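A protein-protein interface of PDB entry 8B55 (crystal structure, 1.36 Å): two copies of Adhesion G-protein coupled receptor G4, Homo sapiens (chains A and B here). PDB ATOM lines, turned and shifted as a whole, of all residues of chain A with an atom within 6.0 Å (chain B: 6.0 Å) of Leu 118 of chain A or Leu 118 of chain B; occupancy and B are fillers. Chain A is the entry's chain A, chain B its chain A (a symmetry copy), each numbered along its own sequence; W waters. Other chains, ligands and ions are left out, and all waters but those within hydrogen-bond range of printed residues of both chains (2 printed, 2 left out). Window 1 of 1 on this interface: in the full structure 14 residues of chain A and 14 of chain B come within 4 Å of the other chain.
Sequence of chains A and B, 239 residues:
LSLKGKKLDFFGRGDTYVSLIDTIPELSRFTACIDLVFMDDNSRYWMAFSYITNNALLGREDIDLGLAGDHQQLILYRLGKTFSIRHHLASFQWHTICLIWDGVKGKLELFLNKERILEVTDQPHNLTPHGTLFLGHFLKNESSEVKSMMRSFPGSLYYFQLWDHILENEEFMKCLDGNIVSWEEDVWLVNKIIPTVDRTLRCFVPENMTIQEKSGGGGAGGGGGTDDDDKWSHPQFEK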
ATOM      1  N   LEU A  76      27.864 -18.538  20.778  1.00  0.00           N
ATOM      2  CA  LEU A  76      27.156 -17.291  21.027  1.00  0.00           C
ATOM      3  C   LEU A  76      27.960 -16.465  22.000  1.00  0.00           C
ATOM      4  O   LEU A  76      28.388 -16.973  23.040  1.00  0.00           O
ATOM      5  CB  LEU A  76      25.787 -17.560  21.647  1.00  0.00           C
ATOM      6  CG  LEU A  76      24.621 -17.946  20.768  1.00  0.00           C
ATOM      7  CD1 LEU A  76      23.358 -18.016  21.666  1.00  0.00           C
ATOM      8  CD2 LEU A  76      24.413 -16.956  19.637  1.00  0.00           C
ATOM      9  N   PHE A  83      28.928 -19.039  24.965  1.00  0.00           N
ATOM     10  CA  PHE A  83      28.140 -20.251  25.106  1.00  0.00           C
ATOM     11  C   PHE A  83      28.354 -21.026  23.831  1.00  0.00           C
ATOM     12  O   PHE A  83      28.077 -20.511  22.750  1.00  0.00           O
ATOM     13  CB  PHE A  83      26.671 -19.903  25.297  1.00  0.00           C
ATOM     14  CG  PHE A  83      26.454 -18.933  26.390  1.00  0.00           C
ATOM     15  CD1 PHE A  83      26.382 -19.368  27.702  1.00  0.00           C
ATOM     16  CD2 PHE A  83      26.363 -17.584  26.130  1.00  0.00           C
ATOM     17  CE1 PHE A  83      26.204 -18.470  28.737  1.00  0.00           C
ATOM     18  CE2 PHE A  83      26.172 -16.685  27.158  1.00  0.00           C
ATOM     19  CZ  PHE A  83      26.098 -17.110  28.439  1.00  0.00           C
ATOM     20  N   SER A  84      28.876 -22.242  23.943  1.00  0.00           N
ATOM     21  CA  SER A  84      29.221 -23.041  22.777  1.00  0.00           C
ATOM     22  C   SER A  84      28.489 -24.371  22.844  1.00  0.00           C
ATOM     23  O   SER A  84      28.424 -24.998  23.907  1.00  0.00           O
ATOM     24  CB  SER A  84      30.729 -23.326  22.709  1.00  0.00           C
ATOM     25  OG  SER A  84      31.493 -22.133  22.867  1.00  0.00           O
ATOM     26  N   ILE A  85      27.943 -24.804  21.702  1.00  0.00           N
ATOM     27  CA  ILE A  85      27.244 -26.075  21.583  1.00  0.00           C
ATOM     28  C   ILE A  85      27.792 -26.814  20.375  1.00  0.00           C
ATOM     29  O   ILE A  85      28.186 -26.204  19.377  1.00  0.00           O
ATOM     30  CB  ILE A  85      25.719 -25.898  21.460  1.00  0.00           C
ATOM     31  CG1 ILE A  85      25.380 -24.922  20.345  1.00  0.00           C
ATOM     32  CG2 ILE A  85      25.144 -25.407  22.770  1.00  0.00           C
ATOM     33  CD1 ILE A  85      23.909 -24.911  19.988  1.00  0.00           C
ATOM     34  N   ARG A  86      27.845 -28.130  20.478  1.00  0.00           N
ATOM     35  CA  ARG A  86      28.216 -28.946  19.332  1.00  0.00           C
ATOM     36  C   ARG A  86      27.106 -28.909  18.278  1.00  0.00           C
ATOM     37  O   ARG A  86      25.919 -29.006  18.606  1.00  0.00           O
ATOM     38  CB  ARG A  86      28.442 -30.389  19.800  1.00  0.00           C
ATOM     39  CG  ARG A  86      28.981 -31.322  18.728  1.00  0.00           C
ATOM     40  CD  ARG A  86      29.250 -32.723  19.261  1.00  0.00           C
ATOM     41  NE  ARG A  86      28.015 -33.469  19.490  1.00  0.00           N
ATOM     42  CZ  ARG A  86      27.961 -34.764  19.781  1.00  0.00           C
ATOM     43  NH1 ARG A  86      29.061 -35.492  19.900  1.00  0.00           N
ATOM     44  NH2 ARG A  86      26.776 -35.343  19.952  1.00  0.00           N
ATOM     45  N   LEU A 108      18.482 -16.231  26.972  1.00  0.00           N
ATOM     46  CA  LEU A 108      19.033 -16.176  25.618  1.00  0.00           C
ATOM     47  C   LEU A 108      18.826 -17.545  24.987  1.00  0.00           C
ATOM     48  O   LEU A 108      19.240 -18.559  25.554  1.00  0.00           O
ATOM     49  CB  LEU A 108      20.526 -15.845  25.672  1.00  0.00           C
ATOM     50  CG  LEU A 108      21.249 -15.669  24.340  1.00  0.00           C
ATOM     51  CD1 LEU A 108      20.775 -14.379  23.680  1.00  0.00           C
ATOM     52  CD2 LEU A 108      22.769 -15.626  24.524  1.00  0.00           C
ATOM     53  N   GLU A 109      18.179 -17.570  23.821  1.00  0.00           N
ATOM     54  CA  GLU A 109      17.876 -18.815  23.123  1.00  0.00           C
ATOM     55  C   GLU A 109      18.428 -18.788  21.706  1.00  0.00           C
ATOM     56  O   GLU A 109      18.451 -17.735  21.057  1.00  0.00           O
ATOM     57  CB  GLU A 109      16.368 -19.052  23.014  1.00  0.00           C
ATOM     58  CG  GLU A 109      15.640 -19.207  24.322  1.00  0.00           C
ATOM     59  CD  GLU A 109      14.140 -19.153  24.138  1.00  0.00           C
ATOM     60  OE1 GLU A 109      13.600 -18.091  23.748  1.00  0.00           O
ATOM     61  OE2 GLU A 109      13.505 -20.188  24.340  1.00  0.00           O
ATOM     62  N   LEU A 110      18.850 -19.964  21.235  1.00  0.00           N
ATOM     63  CA  LEU A 110      19.351 -20.152  19.883  1.00  0.00           C
ATOM     64  C   LEU A 110      18.516 -21.208  19.188  1.00  0.00           C
ATOM     65  O   LEU A 110      18.274 -22.273  19.757  1.00  0.00           O
ATOM     66  CB  LEU A 110      20.817 -20.568  19.922  1.00  0.00           C
ATOM     67  CG  LEU A 110      21.594 -20.542  18.602  1.00  0.00           C
ATOM     68  CD1 LEU A 110      21.657 -19.148  18.047  1.00  0.00           C
ATOM     69  CD2 LEU A 110      23.008 -21.091  18.838  1.00  0.00           C
ATOM     70  N   PHE A 111      18.097 -20.906  17.968  1.00  0.00           N
ATOM     71  CA  PHE A 111      17.289 -21.795  17.153  1.00  0.00           C
ATOM     72  C   PHE A 111      17.970 -22.102  15.831  1.00  0.00           C
ATOM     73  O   PHE A 111      18.616 -21.244  15.247  1.00  0.00           O
ATOM     74  CB  PHE A 111      15.921 -21.178  16.825  1.00  0.00           C
ATOM     75  CG  PHE A 111      15.088 -20.880  18.020  1.00  0.00           C
ATOM     76  CD1 PHE A 111      15.351 -19.765  18.778  1.00  0.00           C
ATOM     77  CD2 PHE A 111      14.035 -21.699  18.364  1.00  0.00           C
ATOM     78  CE1 PHE A 111      14.594 -19.470  19.878  1.00  0.00           C
ATOM     79  CE2 PHE A 111      13.256 -21.422  19.464  1.00  0.00           C
ATOM     80  CZ  PHE A 111      13.532 -20.305  20.239  1.00  0.00           C
ATOM     81  N   ARG A 116      14.565 -25.118  18.756  1.00  0.00           N
ATOM     82  CA  ARG A 116      15.480 -24.568  19.743  1.00  0.00           C
ATOM     83  C   ARG A 116      16.621 -25.547  19.989  1.00  0.00           C
ATOM     84  O   ARG A 116      16.392 -26.732  20.206  1.00  0.00           O
ATOM     85  CB  ARG A 116      14.771 -24.223  21.059  1.00  0.00           C
ATOM     86  CG  ARG A 116      15.696 -23.368  21.939  1.00  0.00           C
ATOM     87  CD  ARG A 116      15.035 -22.906  23.186  1.00  0.00           C
ATOM     88  NE  ARG A 116      14.980 -23.979  24.152  1.00  0.00           N
ATOM     89  CZ  ARG A 116      14.311 -23.902  25.292  1.00  0.00           C
ATOM     90  NH1 ARG A 116      13.642 -22.807  25.626  1.00  0.00           N
ATOM     91  NH2 ARG A 116      14.321 -24.943  26.116  1.00  0.00           N
ATOM     92  N   ILE A 117      17.855 -25.053  19.949  1.00  0.00           N
ATOM     93  CA  ILE A 117      19.013 -25.886  20.240  1.00  0.00           C
ATOM     94  C   ILE A 117      19.741 -25.473  21.514  1.00  0.00           C
ATOM     95  O   ILE A 117      20.519 -26.279  22.048  1.00  0.00           O
ATOM     96  CB  ILE A 117      19.982 -25.990  19.042  1.00  0.00           C
ATOM     97  CG1 ILE A 117      20.468 -24.607  18.619  1.00  0.00           C
ATOM     98  CG2 ILE A 117      19.290 -26.687  17.876  1.00  0.00           C
ATOM     99  CD1 ILE A 117      21.525 -24.631  17.504  1.00  0.00           C
ATOM    100  N   LEU A 118      19.513 -24.265  22.022  1.00  0.00           N
ATOM    101  CA  LEU A 118      20.162 -23.797  23.236  1.00  0.00           C
ATOM    102  C   LEU A 118      19.252 -22.793  23.942  1.00  0.00           C
ATOM    103  O   LEU A 118      18.683 -21.889  23.313  1.00  0.00           O
ATOM    104  CB  LEU A 118      21.514 -23.144  22.914  1.00  0.00           C
ATOM    105  CG  LEU A 118      22.260 -22.490  24.062  1.00  0.00           C
ATOM    106  CD1 LEU A 118      22.802 -23.534  25.033  1.00  0.00           C
ATOM    107  CD2 LEU A 118      23.392 -21.630  23.534  1.00  0.00           C
ATOM    108  N   GLU A 119      19.138 -22.955  25.248  1.00  0.00           N
ATOM    109  CA  GLU A 119      18.601 -21.924  26.117  1.00  0.00           C
ATOM    110  C   GLU A 119      19.583 -21.690  27.257  1.00  0.00           C
ATOM    111  O   GLU A 119      19.964 -22.630  27.955  1.00  0.00           O
ATOM    112  CB  GLU A 119      17.273 -22.364  26.731  1.00  0.00           C
ATOM    113  CG  GLU A 119      16.622 -21.286  27.585  1.00  0.00           C
ATOM    114  CD  GLU A 119      15.530 -21.857  28.467  1.00  0.00           C
ATOM    115  OE1 GLU A 119      15.837 -22.749  29.275  1.00  0.00           O
ATOM    116  OE2 GLU A 119      14.373 -21.439  28.353  1.00  0.00           O
ATOM    117  N   VAL A 120      19.962 -20.432  27.450  1.00  0.00           N
ATOM    118  CA  VAL A 120      20.923 -20.057  28.468  1.00  0.00           C
ATOM    119  C   VAL A 120      20.286 -19.000  29.352  1.00  0.00           C
ATOM    120  O   VAL A 120      19.459 -18.192  28.916  1.00  0.00           O
ATOM    121  CB  VAL A 120      22.215 -19.553  27.782  1.00  0.00           C
ATOM    122  CG1 VAL A 120      22.958 -18.600  28.678  1.00  0.00           C
ATOM    123  CG2 VAL A 120      23.092 -20.733  27.377  1.00  0.00           C
ATOM    124  N   LEU B  76      21.119 -28.427  32.478  1.00  0.00           N
ATOM    125  CA  LEU B  76      22.062 -28.245  33.571  1.00  0.00           C
ATOM    126  C   LEU B  76      21.581 -27.111  34.441  1.00  0.00           C
ATOM    127  O   LEU B  76      21.245 -26.038  33.932  1.00  0.00           O
ATOM    128  CB  LEU B  76      23.446 -27.884  33.039  1.00  0.00           C
ATOM    129  CG  LEU B  76      24.370 -28.967  32.536  1.00  0.00           C
ATOM    130  CD1 LEU B  76      25.731 -28.304  32.196  1.00  0.00           C
ATOM    131  CD2 LEU B  76      24.560 -30.069  33.561  1.00  0.00           C
ATOM    132  N   PHE B  83      20.677 -24.147  31.842  1.00  0.00           N
ATOM    133  CA  PHE B  83      21.256 -24.201  30.512  1.00  0.00           C
ATOM    134  C   PHE B  83      20.709 -25.455  29.879  1.00  0.00           C
ATOM    135  O   PHE B  83      20.892 -26.542  30.423  1.00  0.00           O
ATOM    136  CB  PHE B  83      22.775 -24.249  30.602  1.00  0.00           C
ATOM    137  CG  PHE B  83      23.329 -23.166  31.439  1.00  0.00           C
ATOM    138  CD1 PHE B  83      23.536 -21.907  30.901  1.00  0.00           C
ATOM    139  CD2 PHE B  83      23.607 -23.375  32.772  1.00  0.00           C
ATOM    140  CE1 PHE B  83      24.031 -20.878  31.678  1.00  0.00           C
ATOM    141  CE2 PHE B  83      24.114 -22.354  33.548  1.00  0.00           C
ATOM    142  CZ  PHE B  83      24.320 -21.126  33.022  1.00  0.00           C
ATOM    143  N   SER B  84      20.010 -25.312  28.759  1.00  0.00           N
ATOM    144  CA  SER B  84      19.350 -26.437  28.116  1.00  0.00           C
ATOM    145  C   SER B  84      19.843 -26.559  26.684  1.00  0.00           C
ATOM    146  O   SER B  84      19.969 -25.553  25.977  1.00  0.00           O
ATOM    147  CB  SER B  84      17.824 -26.258  28.085  1.00  0.00           C
ATOM    148  OG  SER B  84      17.312 -25.915  29.370  1.00  0.00           O
ATOM    149  N   ILE B  85      20.115 -27.797  26.255  1.00  0.00           N
ATOM    150  CA  ILE B  85      20.554 -28.094  24.901  1.00  0.00           C
ATOM    151  C   ILE B  85      19.700 -29.222  24.352  1.00  0.00           C
ATOM    152  O   ILE B  85      19.262 -30.108  25.090  1.00  0.00           O
ATOM    153  CB  ILE B  85      22.047 -28.469  24.837  1.00  0.00           C
ATOM    154  CG1 ILE B  85      22.364 -29.579  25.826  1.00  0.00           C
ATOM    155  CG2 ILE B  85      22.903 -27.255  25.129  1.00  0.00           C
ATOM    156  CD1 ILE B  85      23.739 -30.182  25.626  1.00  0.00           C
ATOM    157  N   ARG B  86      19.438 -29.174  23.058  1.00  0.00           N
ATOM    158  CA  ARG B  86      18.752 -30.276  22.402  1.00  0.00           C
ATOM    159  C   ARG B  86      19.667 -31.502  22.337  1.00  0.00           C
ATOM    160  O   ARG B  86      20.856 -31.388  22.025  1.00  0.00           O
ATOM    161  CB  ARG B  86      18.360 -29.844  20.983  1.00  0.00           C
ATOM    162  CG  ARG B  86      17.502 -30.850  20.233  1.00  0.00           C
ATOM    163  CD  ARG B  86      17.086 -30.344  18.858  1.00  0.00           C
ATOM    164  NE  ARG B  86      18.196 -30.366  17.906  1.00  0.00           N
ATOM    165  CZ  ARG B  86      18.071 -30.149  16.602  1.00  0.00           C
ATOM    166  NH1 ARG B  86      16.897 -29.877  16.054  1.00  0.00           N
ATOM    167  NH2 ARG B  86      19.151 -30.212  15.827  1.00  0.00           N
ATOM    168  N   LEU B 108      31.635 -23.839  32.765  1.00  0.00           N
ATOM    169  CA  LEU B 108      30.890 -25.073  33.010  1.00  0.00           C
ATOM    170  C   LEU B 108      30.753 -25.794  31.677  1.00  0.00           C
ATOM    171  O   LEU B 108      30.268 -25.212  30.703  1.00  0.00           O
ATOM    172  CB  LEU B 108      29.505 -24.748  33.573  1.00  0.00           C
ATOM    173  CG  LEU B 108      28.617 -25.926  33.963  1.00  0.00           C
ATOM    174  CD1 LEU B 108      29.193 -26.597  35.205  1.00  0.00           C
ATOM    175  CD2 LEU B 108      27.177 -25.482  34.237  1.00  0.00           C
ATOM    176  N   GLU B 109      31.189 -27.054  31.635  1.00  0.00           N
ATOM    177  CA  GLU B 109      31.156 -27.851  30.413  1.00  0.00           C
ATOM    178  C   GLU B 109      30.395 -29.149  30.635  1.00  0.00           C
ATOM    179  O   GLU B 109      30.449 -29.735  31.724  1.00  0.00           O
ATOM    180  CB  GLU B 109      32.564 -28.228  29.944  1.00  0.00           C
ATOM    181  CG  GLU B 109      33.456 -27.075  29.576  1.00  0.00           C
ATOM    182  CD  GLU B 109      34.892 -27.511  29.400  1.00  0.00           C
ATOM    183  OE1 GLU B 109      35.536 -27.938  30.387  1.00  0.00           O
ATOM    184  OE2 GLU B 109      35.364 -27.470  28.264  1.00  0.00           O
ATOM    185  N   LEU B 110      29.707 -29.595  29.582  1.00  0.00           N
ATOM    186  CA  LEU B 110      28.968 -30.848  29.579  1.00  0.00           C
ATOM    187  C   LEU B 110      29.485 -31.725  28.457  1.00  0.00           C
ATOM    188  O   LEU B 110      29.630 -31.256  27.327  1.00  0.00           O
ATOM    189  CB  LEU B 110      27.479 -30.576  29.404  1.00  0.00           C
ATOM    190  CG  LEU B 110      26.515 -31.740  29.655  1.00  0.00           C
ATOM    191  CD1 LEU B 110      26.604 -32.211  31.078  1.00  0.00           C
ATOM    192  CD2 LEU B 110      25.085 -31.290  29.325  1.00  0.00           C
ATOM    193  N   PHE B 111      29.748 -32.983  28.778  1.00  0.00           N
ATOM    194  CA  PHE B 111      30.248 -33.966  27.833  1.00  0.00           C
ATOM    195  C   PHE B 111      29.320 -35.164  27.741  1.00  0.00           C
ATOM    196  O   PHE B 111      28.746 -35.587  28.733  1.00  0.00           O
ATOM    197  CB  PHE B 111      31.630 -34.495  28.244  1.00  0.00           C
ATOM    198  CG  PHE B 111      32.684 -33.449  28.313  1.00  0.00           C
ATOM    199  CD1 PHE B 111      32.743 -32.605  29.396  1.00  0.00           C
ATOM    200  CD2 PHE B 111      33.623 -33.329  27.311  1.00  0.00           C
ATOM    201  CE1 PHE B 111      33.707 -31.639  29.482  1.00  0.00           C
ATOM    202  CE2 PHE B 111      34.605 -32.369  27.375  1.00  0.00           C
ATOM    203  CZ  PHE B 111      34.654 -31.506  28.461  1.00  0.00           C
ATOM    204  N   ARG B 116      32.584 -33.012  24.003  1.00  0.00           N
ATOM    205  CA  ARG B 116      31.948 -31.858  24.618  1.00  0.00           C
ATOM    206  C   ARG B 116      30.712 -31.465  23.821  1.00  0.00           C
ATOM    207  O   ARG B 116      30.764 -31.346  22.602  1.00  0.00           O
ATOM    208  CB  ARG B 116      32.910 -30.669  24.744  1.00  0.00           C
ATOM    209  CG  ARG B 116      32.301 -29.604  25.669  1.00  0.00           C
ATOM    210  CD  ARG B 116      33.223 -28.469  25.924  1.00  0.00           C
ATOM    211  NE  ARG B 116      33.249 -27.578  24.786  1.00  0.00           N
ATOM    212  CZ  ARG B 116      34.095 -26.568  24.668  1.00  0.00           C
ATOM    213  NH1 ARG B 116      34.989 -26.303  25.612  1.00  0.00           N
ATOM    214  NH2 ARG B 116      34.040 -25.804  23.584  1.00  0.00           N
ATOM    215  N   ILE B 117      29.591 -31.269  24.509  1.00  0.00           N
ATOM    216  CA  ILE B 117      28.369 -30.823  23.855  1.00  0.00           C
ATOM    217  C   ILE B 117      27.938 -29.425  24.284  1.00  0.00           C
ATOM    218  O   ILE B 117      27.129 -28.803  23.577  1.00  0.00           O
ATOM    219  CB  ILE B 117      27.215 -31.840  24.000  1.00  0.00           C
ATOM    220  CG1 ILE B 117      26.914 -32.109  25.471  1.00  0.00           C
ATOM    221  CG2 ILE B 117      27.579 -33.139  23.290  1.00  0.00           C
ATOM    222  CD1 ILE B 117      25.702 -33.024  25.702  1.00  0.00           C
ATOM    223  N   LEU B 118      28.449 -28.908  25.398  1.00  0.00           N
ATOM    224  CA  LEU B 118      28.097 -27.579  25.872  1.00  0.00           C
ATOM    225  C   LEU B 118      29.268 -26.995  26.660  1.00  0.00           C
ATOM    226  O   LEU B 118      29.874 -27.669  27.505  1.00  0.00           O
ATOM    227  CB  LEU B 118      26.844 -27.633  26.757  1.00  0.00           C
ATOM    228  CG  LEU B 118      26.415 -26.344  27.436  1.00  0.00           C
ATOM    229  CD1 LEU B 118      25.867 -25.344  26.423  1.00  0.00           C
ATOM    230  CD2 LEU B 118      25.378 -26.629  28.504  1.00  0.00           C
ATOM    231  N   GLU B 119      29.562 -25.736  26.385  1.00  0.00           N
ATOM    232  CA  GLU B 119      30.401 -24.926  27.246  1.00  0.00           C
ATOM    233  C   GLU B 119      29.671 -23.624  27.550  1.00  0.00           C
ATOM    234  O   GLU B 119      29.252 -22.915  26.634  1.00  0.00           O
ATOM    235  CB  GLU B 119      31.715 -24.570  26.553  1.00  0.00           C
ATOM    236  CG  GLU B 119      32.672 -23.791  27.443  1.00  0.00           C
ATOM    237  CD  GLU B 119      33.778 -23.138  26.639  1.00  0.00           C
ATOM    238  OE1 GLU B 119      33.456 -22.332  25.751  1.00  0.00           O
ATOM    239  OE2 GLU B 119      34.954 -23.430  26.872  1.00  0.00           O
ATOM    240  N   VAL B 120      29.552 -23.310  28.834  1.00  0.00           N
ATOM    241  CA  VAL B 120      28.847 -22.126  29.283  1.00  0.00           C
ATOM    242  C   VAL B 120      29.790 -21.316  30.154  1.00  0.00           C
ATOM    243  O   VAL B 120      30.663 -21.849  30.847  1.00  0.00           O
ATOM    244  CB  VAL B 120      27.567 -22.554  30.039  1.00  0.00           C
ATOM    245  CG1 VAL B 120      27.154 -21.500  31.030  1.00  0.00           C
ATOM    246  CG2 VAL B 120      26.446 -22.858  29.051  1.00  0.00           C
HETATM  247  O   HOH W   1      22.224 -28.621  21.210  1.00  0.00           O
HETATM  248  O   HOH W   2      24.935 -29.444  21.611  1.00  0.00           O
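The backbone carbonyl oxygen of Glu 119 of chain A sits at hydrogen-bond distance from the backbone NH of Ser 84 of chain B. The backbone NH (N) of Arg 86 of chain A lies within hydrogen-bond range of the backbone carbonyl oxygen (O) of Ile 117 of chain B (3.3 Å). O of Ile 117 of chain A sits at hydrogen-bond distance from N of Arg 86 of chain B (3.3 Å). The backbone NH (N) of Ser 84 of chain A is in hydrogen-bond range of the backbone carbonyl oxygen (O) of Glu 119 of chain B (2.8 Å).
The backbone NH (N) of Val 120 of chain A sits at hydrogen-bond distance from the backbone carbonyl oxygen (O) of Leu 108 of chain A (2.8 Å). NH1 of Arg 116 of chain B lies within salt-bridge range of OE2 of Glu 119 of chain B. N of Leu 110 of chain A is in hydrogen-bond range of O of Leu 118 of chain A (2.8 Å). OE2 of Glu 109 of chain B is in salt-bridge range of NH1 of Arg 116 of chain B, at 2.9 Å. The backbone NH of Ile 117 of chain A is in hydrogen-bond range of the backbone carbonyl oxygen of Leu 110 of chain A (2.8 Å). N of Leu 110 of chain B sits at hydrogen-bond distance from O of Leu 118 of chain B (2.8 Å).
CA of Phe 83 of chain A touches O of Glu 119 of chain B (3.3 Å). Phe 83 of chain A touches Val 120 of chain B (CD1 to CG2, 3.7 Å). Ile 85 of chain A touches Ile 85 of chain B (CG2 to CG2, 3.7 Å). Ile 117 of chain B touches Ile 85 of chain A (O to CA, 3.4 Å). Arg 86 of chain A touches Arg 116 of chain B. O of Arg 116 of chain A touches CB of Arg 86 of chain B, 3.8 Å away. CD1 of Leu 118 of chain A touches CG2 of Ile 85 of chain B, at 3.7 Å. Leu 118 of chain A touches Leu 118 of chain B. Glu 119 of chain A touches Phe 83 of chain B (O to CA, 3.3 Å). Val 120 of chain A touches Phe 83 of chain B.
Leu 118 of chain A touches just these residues of chain B: Ser 84, Ile 85 and Leu 118. Printed residues of chain A within 4 Å of Arg 116 of chain B: Arg 86. Printed residues of chain B within 4 Å of Ile 117 of chain A: Ile 85 (3.4 Å) and Arg 86 (3.3 Å). Printed residues of chain B within 4 Å of Glu 119 of chain A: Phe 83 (3.3 Å) and Ser 84 (2.8 Å). Printed residues of chain B within 4 Å of Val 120 of chain A: Phe 83. Of the printed residues of chain B, Phe 83 of chain A touches Glu 119 and Val 120. Leu 108 of chain B touches none of the printed residues of chain A. The nearest residue of chain B that does not touch Leu 118 of chain A is Arg 86 of chain B (5.0 Å). The nearest residue of chain A that does not touch Leu 118 of chain B is Arg 86 of chain A (5.0 Å). The nearest printed residue of chain B that does not touch Ile 85 of chain A is Glu 119 of chain B (5.0 Å).
Printed residues of chain A that touch a printed residue of chain B: Phe 83, Ser 84, Ile 85, Arg 86, Arg 116, Ile 117, Leu 118, Glu 119 and Val 120. Among the printed residues, no Asp or Glu carboxylate lies within 4 Å of a Lys or Arg side-chain nitrogen of the other chain.
Ser 84 of chain A touches Leu 118 of chain B, and with the chains exchanged Leu 118 of chain A touches Ser 84 of chain B. Ser 84 of chain A touches Glu 119 of chain B, and with the chains exchanged Glu 119 of chain A touches Ser 84 of chain B. Ile 85 of chain A touches Ile 117 of chain B, and with the chains exchanged Ile 117 of chain A touches Ile 85 of chain B. Arg 86 of chain A touches Arg 116 of chain B, and with the chains exchanged Arg 116 of chain A touches Arg 86 of chain B.
Water W2 bridges the backbone carbonyl oxygen of Ile 117 of chain B (3.0 Å) and the backbone carbonyl oxygen of Arg 86 of chain A (3.2 Å). Water W1 lies within hydrogen-bond range of the backbone carbonyl oxygen (O) of Ile 117 of chain A (3.0 Å) and the backbone carbonyl oxygen (O) of Arg 86 of chain B (3.2 Å).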
